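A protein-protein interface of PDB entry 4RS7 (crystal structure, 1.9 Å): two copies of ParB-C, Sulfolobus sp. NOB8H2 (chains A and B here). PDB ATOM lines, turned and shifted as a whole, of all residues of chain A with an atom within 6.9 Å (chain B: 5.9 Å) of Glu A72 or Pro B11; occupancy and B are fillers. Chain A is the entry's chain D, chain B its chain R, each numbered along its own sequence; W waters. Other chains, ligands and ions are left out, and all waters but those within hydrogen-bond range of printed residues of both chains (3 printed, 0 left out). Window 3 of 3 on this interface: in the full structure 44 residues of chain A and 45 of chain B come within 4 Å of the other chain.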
ATOM      1  N   GLU A  67      14.879   1.555 -15.617  1.00  0.00           N
ATOM      2  CA  GLU A  67      14.494   1.059 -16.934  1.00  0.00           C
ATOM      3  C   GLU A  67      15.507   0.040 -17.450  1.00  0.00           C
ATOM      4  O   GLU A  67      15.141  -0.974 -18.043  1.00  0.00           O
ATOM      5  CB  GLU A  67      14.350   2.227 -17.919  1.00  0.00           C
ATOM      6  CG  GLU A  67      14.227   1.825 -19.376  1.00  0.00           C
ATOM      7  CD  GLU A  67      13.977   3.016 -20.290  1.00  0.00           C
ATOM      8  OE1 GLU A  67      13.297   3.970 -19.855  1.00  0.00           O
ATOM      9  OE2 GLU A  67      14.463   3.000 -21.441  1.00  0.00           O
ATOM     10  N   GLU A  68      16.786   0.308 -17.222  1.00  0.00           N
ATOM     11  CA  GLU A  68      17.822  -0.636 -17.615  1.00  0.00           C
ATOM     12  C   GLU A  68      17.618  -1.989 -16.949  1.00  0.00           C
ATOM     13  O   GLU A  68      17.791  -3.027 -17.583  1.00  0.00           O
ATOM     14  CB  GLU A  68      19.213  -0.088 -17.292  1.00  0.00           C
ATOM     15  CG  GLU A  68      19.744   0.872 -18.344  1.00  0.00           C
ATOM     16  CD  GLU A  68      21.067   1.491 -17.948  1.00  0.00           C
ATOM     17  OE1 GLU A  68      21.361   1.536 -16.735  1.00  0.00           O
ATOM     18  OE2 GLU A  68      21.813   1.928 -18.849  1.00  0.00           O
ATOM     19  N   ILE A  69      17.253  -1.976 -15.672  1.00  0.00           N
ATOM     20  CA  ILE A  69      17.039  -3.222 -14.942  1.00  0.00           C
ATOM     21  C   ILE A  69      15.823  -3.977 -15.484  1.00  0.00           C
ATOM     22  O   ILE A  69      15.851  -5.202 -15.596  1.00  0.00           O
ATOM     23  CB  ILE A  69      16.955  -2.994 -13.412  1.00  0.00           C
ATOM     24  CG1 ILE A  69      18.307  -2.488 -12.894  1.00  0.00           C
ATOM     25  CG2 ILE A  69      16.573  -4.288 -12.683  1.00  0.00           C
ATOM     26  CD1 ILE A  69      18.379  -2.310 -11.398  1.00  0.00           C
ATOM     27  N   PHE A  70      14.769  -3.247 -15.844  1.00  0.00           N
ATOM     28  CA  PHE A  70      13.608  -3.865 -16.484  1.00  0.00           C
ATOM     29  C   PHE A  70      14.008  -4.622 -17.748  1.00  0.00           C
ATOM     30  O   PHE A  70      13.647  -5.788 -17.929  1.00  0.00           O
ATOM     31  CB  PHE A  70      12.539  -2.819 -16.827  1.00  0.00           C
ATOM     32  CG  PHE A  70      11.386  -3.370 -17.633  1.00  0.00           C
ATOM     33  CD1 PHE A  70      10.361  -4.066 -17.015  1.00  0.00           C
ATOM     34  CD2 PHE A  70      11.335  -3.195 -19.007  1.00  0.00           C
ATOM     35  CE1 PHE A  70       9.297  -4.574 -17.755  1.00  0.00           C
ATOM     36  CE2 PHE A  70      10.274  -3.701 -19.753  1.00  0.00           C
ATOM     37  CZ  PHE A  70       9.258  -4.391 -19.124  1.00  0.00           C
ATOM     38  N   TYR A  71      14.745  -3.958 -18.629  1.00  0.00           N
ATOM     39  CA  TYR A  71      15.167  -4.602 -19.869  1.00  0.00           C
ATOM     40  C   TYR A  71      16.084  -5.787 -19.585  1.00  0.00           C
ATOM     41  O   TYR A  71      16.034  -6.807 -20.274  1.00  0.00           O
ATOM     42  CB  TYR A  71      15.807  -3.594 -20.833  1.00  0.00           C
ATOM     43  CG  TYR A  71      14.783  -2.676 -21.468  1.00  0.00           C
ATOM     44  CD1 TYR A  71      14.667  -1.350 -21.078  1.00  0.00           C
ATOM     45  CD2 TYR A  71      13.907  -3.151 -22.433  1.00  0.00           C
ATOM     46  CE1 TYR A  71      13.717  -0.515 -21.647  1.00  0.00           C
ATOM     47  CE2 TYR A  71      12.957  -2.327 -23.006  1.00  0.00           C
ATOM     48  CZ  TYR A  71      12.865  -1.010 -22.609  1.00  0.00           C
ATOM     49  OH  TYR A  71      11.918  -0.185 -23.179  1.00  0.00           O
ATOM     50  N   GLU A  72      16.911  -5.666 -18.555  1.00  0.00           N
ATOM     51  CA  GLU A  72      17.746  -6.796 -18.161  1.00  0.00           C
ATOM     52  C   GLU A  72      16.870  -7.989 -17.773  1.00  0.00           C
ATOM     53  O   GLU A  72      17.171  -9.130 -18.123  1.00  0.00           O
ATOM     54  CB  GLU A  72      18.676  -6.409 -17.016  1.00  0.00           C
ATOM     55  CG  GLU A  72      19.586  -7.531 -16.550  1.00  0.00           C
ATOM     56  CD  GLU A  72      20.661  -7.027 -15.618  1.00  0.00           C
ATOM     57  OE1 GLU A  72      21.474  -6.188 -16.057  1.00  0.00           O
ATOM     58  OE2 GLU A  72      20.678  -7.448 -14.448  1.00  0.00           O
ATOM     59  N   MET A  73      15.771  -7.714 -17.074  1.00  0.00           N
ATOM     60  CA  MET A  73      14.868  -8.765 -16.605  1.00  0.00           C
ATOM     61  C   MET A  73      14.110  -9.447 -17.750  1.00  0.00           C
ATOM     62  O   MET A  73      13.968 -10.672 -17.773  1.00  0.00           O
ATOM     63  CB  MET A  73      13.868  -8.192 -15.583  1.00  0.00           C
ATOM     64  CG  MET A  73      12.795  -9.185 -15.104  1.00  0.00           C
ATOM     65  SD  MET A  73      11.515  -8.420 -13.835  1.00  0.00           S
ATOM     66  CE  MET A  73      12.685  -8.274 -12.278  1.00  0.00           C
ATOM     67  N   VAL A  74      13.629  -8.658 -18.703  1.00  0.00           N
ATOM     68  CA  VAL A  74      12.677  -9.184 -19.681  1.00  0.00           C
ATOM     69  C   VAL A  74      13.217  -9.401 -21.093  1.00  0.00           C
ATOM     70  O   VAL A  74      12.543 -10.022 -21.912  1.00  0.00           O
ATOM     71  CB  VAL A  74      11.389  -8.326 -19.745  1.00  0.00           C
ATOM     72  CG1 VAL A  74      10.744  -8.256 -18.369  1.00  0.00           C
ATOM     73  CG2 VAL A  74      11.690  -6.926 -20.284  1.00  0.00           C
ATOM     74  N   ARG A  75      14.419  -8.910 -21.383  1.00  0.00           N
ATOM     75  CA  ARG A  75      14.978  -9.070 -22.731  1.00  0.00           C
ATOM     76  C   ARG A  75      14.958 -10.512 -23.237  1.00  0.00           C
ATOM     77  O   ARG A  75      14.613 -10.758 -24.394  1.00  0.00           O
ATOM     78  CB  ARG A  75      16.395  -8.496 -22.837  1.00  0.00           C
ATOM     79  CG  ARG A  75      17.093  -8.820 -24.164  1.00  0.00           C
ATOM     80  CD  ARG A  75      16.209  -8.488 -25.365  1.00  0.00           C
ATOM     81  NE  ARG A  75      16.833  -8.829 -26.646  1.00  0.00           N
ATOM     82  CZ  ARG A  75      16.658  -9.977 -27.299  1.00  0.00           C
ATOM     83  NH1 ARG A  75      15.879 -10.934 -26.804  1.00  0.00           N
ATOM     84  NH2 ARG A  75      17.273 -10.171 -28.458  1.00  0.00           N
ATOM     85  N   PRO A  76      15.347 -11.472 -22.386  1.00  0.00           N
ATOM     86  CA  PRO A  76      15.302 -12.863 -22.845  1.00  0.00           C
ATOM     87  C   PRO A  76      13.884 -13.332 -23.171  1.00  0.00           C
ATOM     88  O   PRO A  76      13.730 -14.366 -23.817  1.00  0.00           O
ATOM     89  CB  PRO A  76      15.851 -13.644 -21.647  1.00  0.00           C
ATOM     90  CG  PRO A  76      16.703 -12.668 -20.923  1.00  0.00           C
ATOM     91  CD  PRO A  76      15.999 -11.348 -21.069  1.00  0.00           C
ATOM     92  N   LEU B   6      18.600 -16.223 -10.268  1.00  0.00           N
ATOM     93  CA  LEU B   6      18.300 -14.808 -10.462  1.00  0.00           C
ATOM     94  C   LEU B   6      19.570 -13.998 -10.714  1.00  0.00           C
ATOM     95  O   LEU B   6      19.622 -13.179 -11.633  1.00  0.00           O
ATOM     96  CB  LEU B   6      17.559 -14.252  -9.246  1.00  0.00           C
ATOM     97  CG  LEU B   6      17.273 -12.750  -9.293  1.00  0.00           C
ATOM     98  CD1 LEU B   6      16.249 -12.439 -10.380  1.00  0.00           C
ATOM     99  CD2 LEU B   6      16.796 -12.245  -7.941  1.00  0.00           C
ATOM    100  N   TYR B   7      20.594 -14.233  -9.900  1.00  0.00           N
ATOM    101  CA  TYR B   7      21.845 -13.486 -10.016  1.00  0.00           C
ATOM    102  C   TYR B   7      22.544 -13.724 -11.349  1.00  0.00           C
ATOM    103  O   TYR B   7      23.137 -12.806 -11.917  1.00  0.00           O
ATOM    104  CB  TYR B   7      22.781 -13.818  -8.855  1.00  0.00           C
ATOM    105  CG  TYR B   7      22.265 -13.357  -7.510  1.00  0.00           C
ATOM    106  CD1 TYR B   7      22.660 -13.990  -6.340  1.00  0.00           C
ATOM    107  CD2 TYR B   7      21.385 -12.286  -7.412  1.00  0.00           C
ATOM    108  CE1 TYR B   7      22.192 -13.573  -5.109  1.00  0.00           C
ATOM    109  CE2 TYR B   7      20.912 -11.860  -6.185  1.00  0.00           C
ATOM    110  CZ  TYR B   7      21.319 -12.510  -5.037  1.00  0.00           C
ATOM    111  OH  TYR B   7      20.856 -12.094  -3.811  1.00  0.00           O
ATOM    112  N   ARG B   8      22.486 -14.956 -11.848  1.00  0.00           N
ATOM    113  CA  ARG B   8      23.069 -15.253 -13.152  1.00  0.00           C
ATOM    114  C   ARG B   8      22.323 -14.523 -14.262  1.00  0.00           C
ATOM    115  O   ARG B   8      22.934 -14.017 -15.208  1.00  0.00           O
ATOM    116  CB  ARG B   8      23.090 -16.761 -13.423  1.00  0.00           C
ATOM    117  CG  ARG B   8      24.239 -17.499 -12.740  1.00  0.00           C
ATOM    118  CD  ARG B   8      24.330 -18.946 -13.208  1.00  0.00           C
ATOM    119  NE  ARG B   8      23.135 -19.706 -12.853  1.00  0.00           N
ATOM    120  CZ  ARG B   8      23.007 -20.425 -11.742  1.00  0.00           C
ATOM    121  NH1 ARG B   8      24.007 -20.490 -10.870  1.00  0.00           N
ATOM    122  NH2 ARG B   8      21.881 -21.084 -11.503  1.00  0.00           N
ATOM    123  N   ALA B   9      21.001 -14.464 -14.139  1.00  0.00           N
ATOM    124  CA  ALA B   9      20.170 -13.821 -15.150  1.00  0.00           C
ATOM    125  C   ALA B   9      20.197 -12.299 -15.033  1.00  0.00           C
ATOM    126  O   ALA B   9      20.056 -11.596 -16.030  1.00  0.00           O
ATOM    127  CB  ALA B   9      18.739 -14.334 -15.069  1.00  0.00           C
ATOM    128  N   MET B  10      20.389 -11.796 -13.816  1.00  0.00           N
ATOM    129  CA  MET B  10      20.345 -10.359 -13.576  1.00  0.00           C
ATOM    130  C   MET B  10      21.553  -9.872 -12.773  1.00  0.00           C
ATOM    131  O   MET B  10      21.466  -9.694 -11.555  1.00  0.00           O
ATOM    132  CB  MET B  10      19.037  -9.976 -12.872  1.00  0.00           C
ATOM    133  CG  MET B  10      17.778 -10.421 -13.624  1.00  0.00           C
ATOM    134  SD  MET B  10      16.145  -9.579 -12.976  1.00  0.00           S
ATOM    135  CE  MET B  10      16.611  -7.719 -13.380  1.00  0.00           C
ATOM    136  N   PRO B  11      22.687  -9.659 -13.460  1.00  0.00           N
ATOM    137  CA  PRO B  11      23.915  -9.164 -12.829  1.00  0.00           C
ATOM    138  C   PRO B  11      23.699  -7.844 -12.094  1.00  0.00           C
ATOM    139  O   PRO B  11      24.382  -7.583 -11.106  1.00  0.00           O
ATOM    140  CB  PRO B  11      24.856  -8.948 -14.019  1.00  0.00           C
ATOM    141  CG  PRO B  11      24.362  -9.872 -15.062  1.00  0.00           C
ATOM    142  CD  PRO B  11      22.874  -9.921 -14.898  1.00  0.00           C
ATOM    143  N   SER B  12      22.765  -7.025 -12.572  1.00  0.00           N
ATOM    144  CA  SER B  12      22.496  -5.730 -11.950  1.00  0.00           C
ATOM    145  C   SER B  12      21.941  -5.892 -10.544  1.00  0.00           C
ATOM    146  O   SER B  12      22.242  -5.097  -9.655  1.00  0.00           O
ATOM    147  CB  SER B  12      21.523  -4.907 -12.795  1.00  0.00           C
ATOM    148  OG  SER B  12      22.132  -4.511 -14.011  1.00  0.00           O
ATOM    149  N   ILE B  13      21.117  -6.917 -10.355  1.00  0.00           N
ATOM    150  CA  ILE B  13      20.511  -7.187  -9.058  1.00  0.00           C
ATOM    151  C   ILE B  13      21.532  -7.784  -8.091  1.00  0.00           C
ATOM    152  O   ILE B  13      21.578  -7.418  -6.913  1.00  0.00           O
ATOM    153  CB  ILE B  13      19.300  -8.129  -9.187  1.00  0.00           C
ATOM    154  CG1 ILE B  13      18.216  -7.481 -10.054  1.00  0.00           C
ATOM    155  CG2 ILE B  13      18.751  -8.480  -7.812  1.00  0.00           C
ATOM    156  CD1 ILE B  13      17.612  -6.220  -9.453  1.00  0.00           C
ATOM    157  N   LYS B  14      22.345  -8.705  -8.597  1.00  0.00           N
ATOM    158  CA  LYS B  14      23.455  -9.256  -7.829  1.00  0.00           C
ATOM    159  C   LYS B  14      24.334  -8.135  -7.278  1.00  0.00           C
ATOM    160  O   LYS B  14      24.683  -8.124  -6.094  1.00  0.00           O
ATOM    161  CB  LYS B  14      24.286 -10.196  -8.703  1.00  0.00           C
ATOM    162  CG  LYS B  14      25.570 -10.690  -8.049  1.00  0.00           C
ATOM    163  CD  LYS B  14      26.242 -11.761  -8.890  1.00  0.00           C
ATOM    164  CE  LYS B  14      27.593 -12.143  -8.314  1.00  0.00           C
ATOM    165  NZ  LYS B  14      27.509 -12.336  -6.847  1.00  0.00           N
ATOM    166  N   LYS B  15      24.686  -7.191  -8.146  1.00  0.00           N
ATOM    167  CA  LYS B  15      25.529  -6.069  -7.756  1.00  0.00           C
ATOM    168  C   LYS B  15      24.883  -5.240  -6.643  1.00  0.00           C
ATOM    169  O   LYS B  15      25.530  -4.912  -5.651  1.00  0.00           O
ATOM    170  CB  LYS B  15      25.852  -5.199  -8.975  1.00  0.00           C
ATOM    171  CG  LYS B  15      26.609  -3.918  -8.661  1.00  0.00           C
ATOM    172  CD  LYS B  15      27.068  -3.232  -9.944  1.00  0.00           C
ATOM    173  CE  LYS B  15      27.795  -1.929  -9.651  1.00  0.00           C
ATOM    174  NZ  LYS B  15      28.670  -1.513 -10.780  1.00  0.00           N
ATOM    175  N   LEU B  16      23.605  -4.909  -6.803  1.00  0.00           N
ATOM    176  CA  LEU B  16      22.897  -4.123  -5.797  1.00  0.00           C
ATOM    177  C   LEU B  16      22.901  -4.805  -4.428  1.00  0.00           C
ATOM    178  O   LEU B  16      23.076  -4.149  -3.404  1.00  0.00           O
ATOM    179  CB  LEU B  16      21.465  -3.809  -6.247  1.00  0.00           C
ATOM    180  CG  LEU B  16      21.324  -2.798  -7.392  1.00  0.00           C
ATOM    181  CD1 LEU B  16      19.878  -2.692  -7.868  1.00  0.00           C
ATOM    182  CD2 LEU B  16      21.857  -1.427  -6.983  1.00  0.00           C
HETATM  183  O   HOH W   1      17.336 -11.875 -17.346  1.00  0.00           O
HETATM  184  O   HOH W   2      21.140  -3.746 -16.344  1.00  0.00           O
HETATM  185  O   HOH W   3      24.657  -5.867 -15.963  1.00  0.00           O
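Hydrophobic or aromatic side chains of chain B that line the printed part of chain A: Met B10, Pro B11, Ile B13 and Leu B16. Of the 10 printed residues of chain A, 3 touch a printed residue of chain B. Printed residues of chain A that touch a printed residue of chain B: Ile A69, Glu A72 and Met A73. Among the printed residues, 7 pairs touch across the chains.
OG of Ser B12 is in hydrogen-bond range of OE1 of Glu A72, at 2.7 Å. OE2 of Glu A72 lies close to N of Pro B11 (3.1 Å).
Water W2 lies within hydrogen-bond range of the side-chain carboxylate of Glu A72 and the side-chain hydroxyl of Ser B12. Water W1 bridges the backbone carbonyl oxygen of Glu A72 (2.9 Å) and the backbone carbonyl oxygen of Ala B9 (3.0 Å). Water W3 lies within hydrogen-bond range of the side-chain carboxylate (OE1) of Glu A72 (3.2 Å) and the side-chain hydroxyl (OG) of Ser B12 (3.5 Å).
No position is printed for both chains. Of the 7 pairs that touch across the chains among the printed residues, none has its exchanged pair printed and touching as well.
Among the printed residues, merely in contact across the chains: Glu A72 with Met B10 (3.1 Å), Ile A69 with Met B10 (3.4 Å), Met A73 with Met B10 (3.5 Å), Ile A69 with Leu B16 (3.9 Å) and Ile A69 with Ile B13 (3.9 Å).
Printed residues of chain B within 4 Å of Ile A69: Met B10 (3.4 Å), Ile B13 (3.9 Å) and Leu B16 (3.9 Å). Glu A72 touches just these residues of chain B: Met B10 (3.1 Å), Pro B11 (3.1 Å) and Ser B12 (2.7 Å). Of the printed residues of chain B, Met A73 touches Met B10. Printed residues of chain A within 4 Å of Pro B11: Glu A72 (3.1 Å). Of the printed residues of chain A, Ile B13 touches Ile A69 (3.9 Å). Of the printed residues of chain A, Leu B16 touches Ile A69. The nearest printed residue of chain A that does not touch Pro B11 is Ile A69 (7.6 Å). The nearest printed residue of chain B that does not touch Ile A69 is Ser B12 (4.03 Å).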
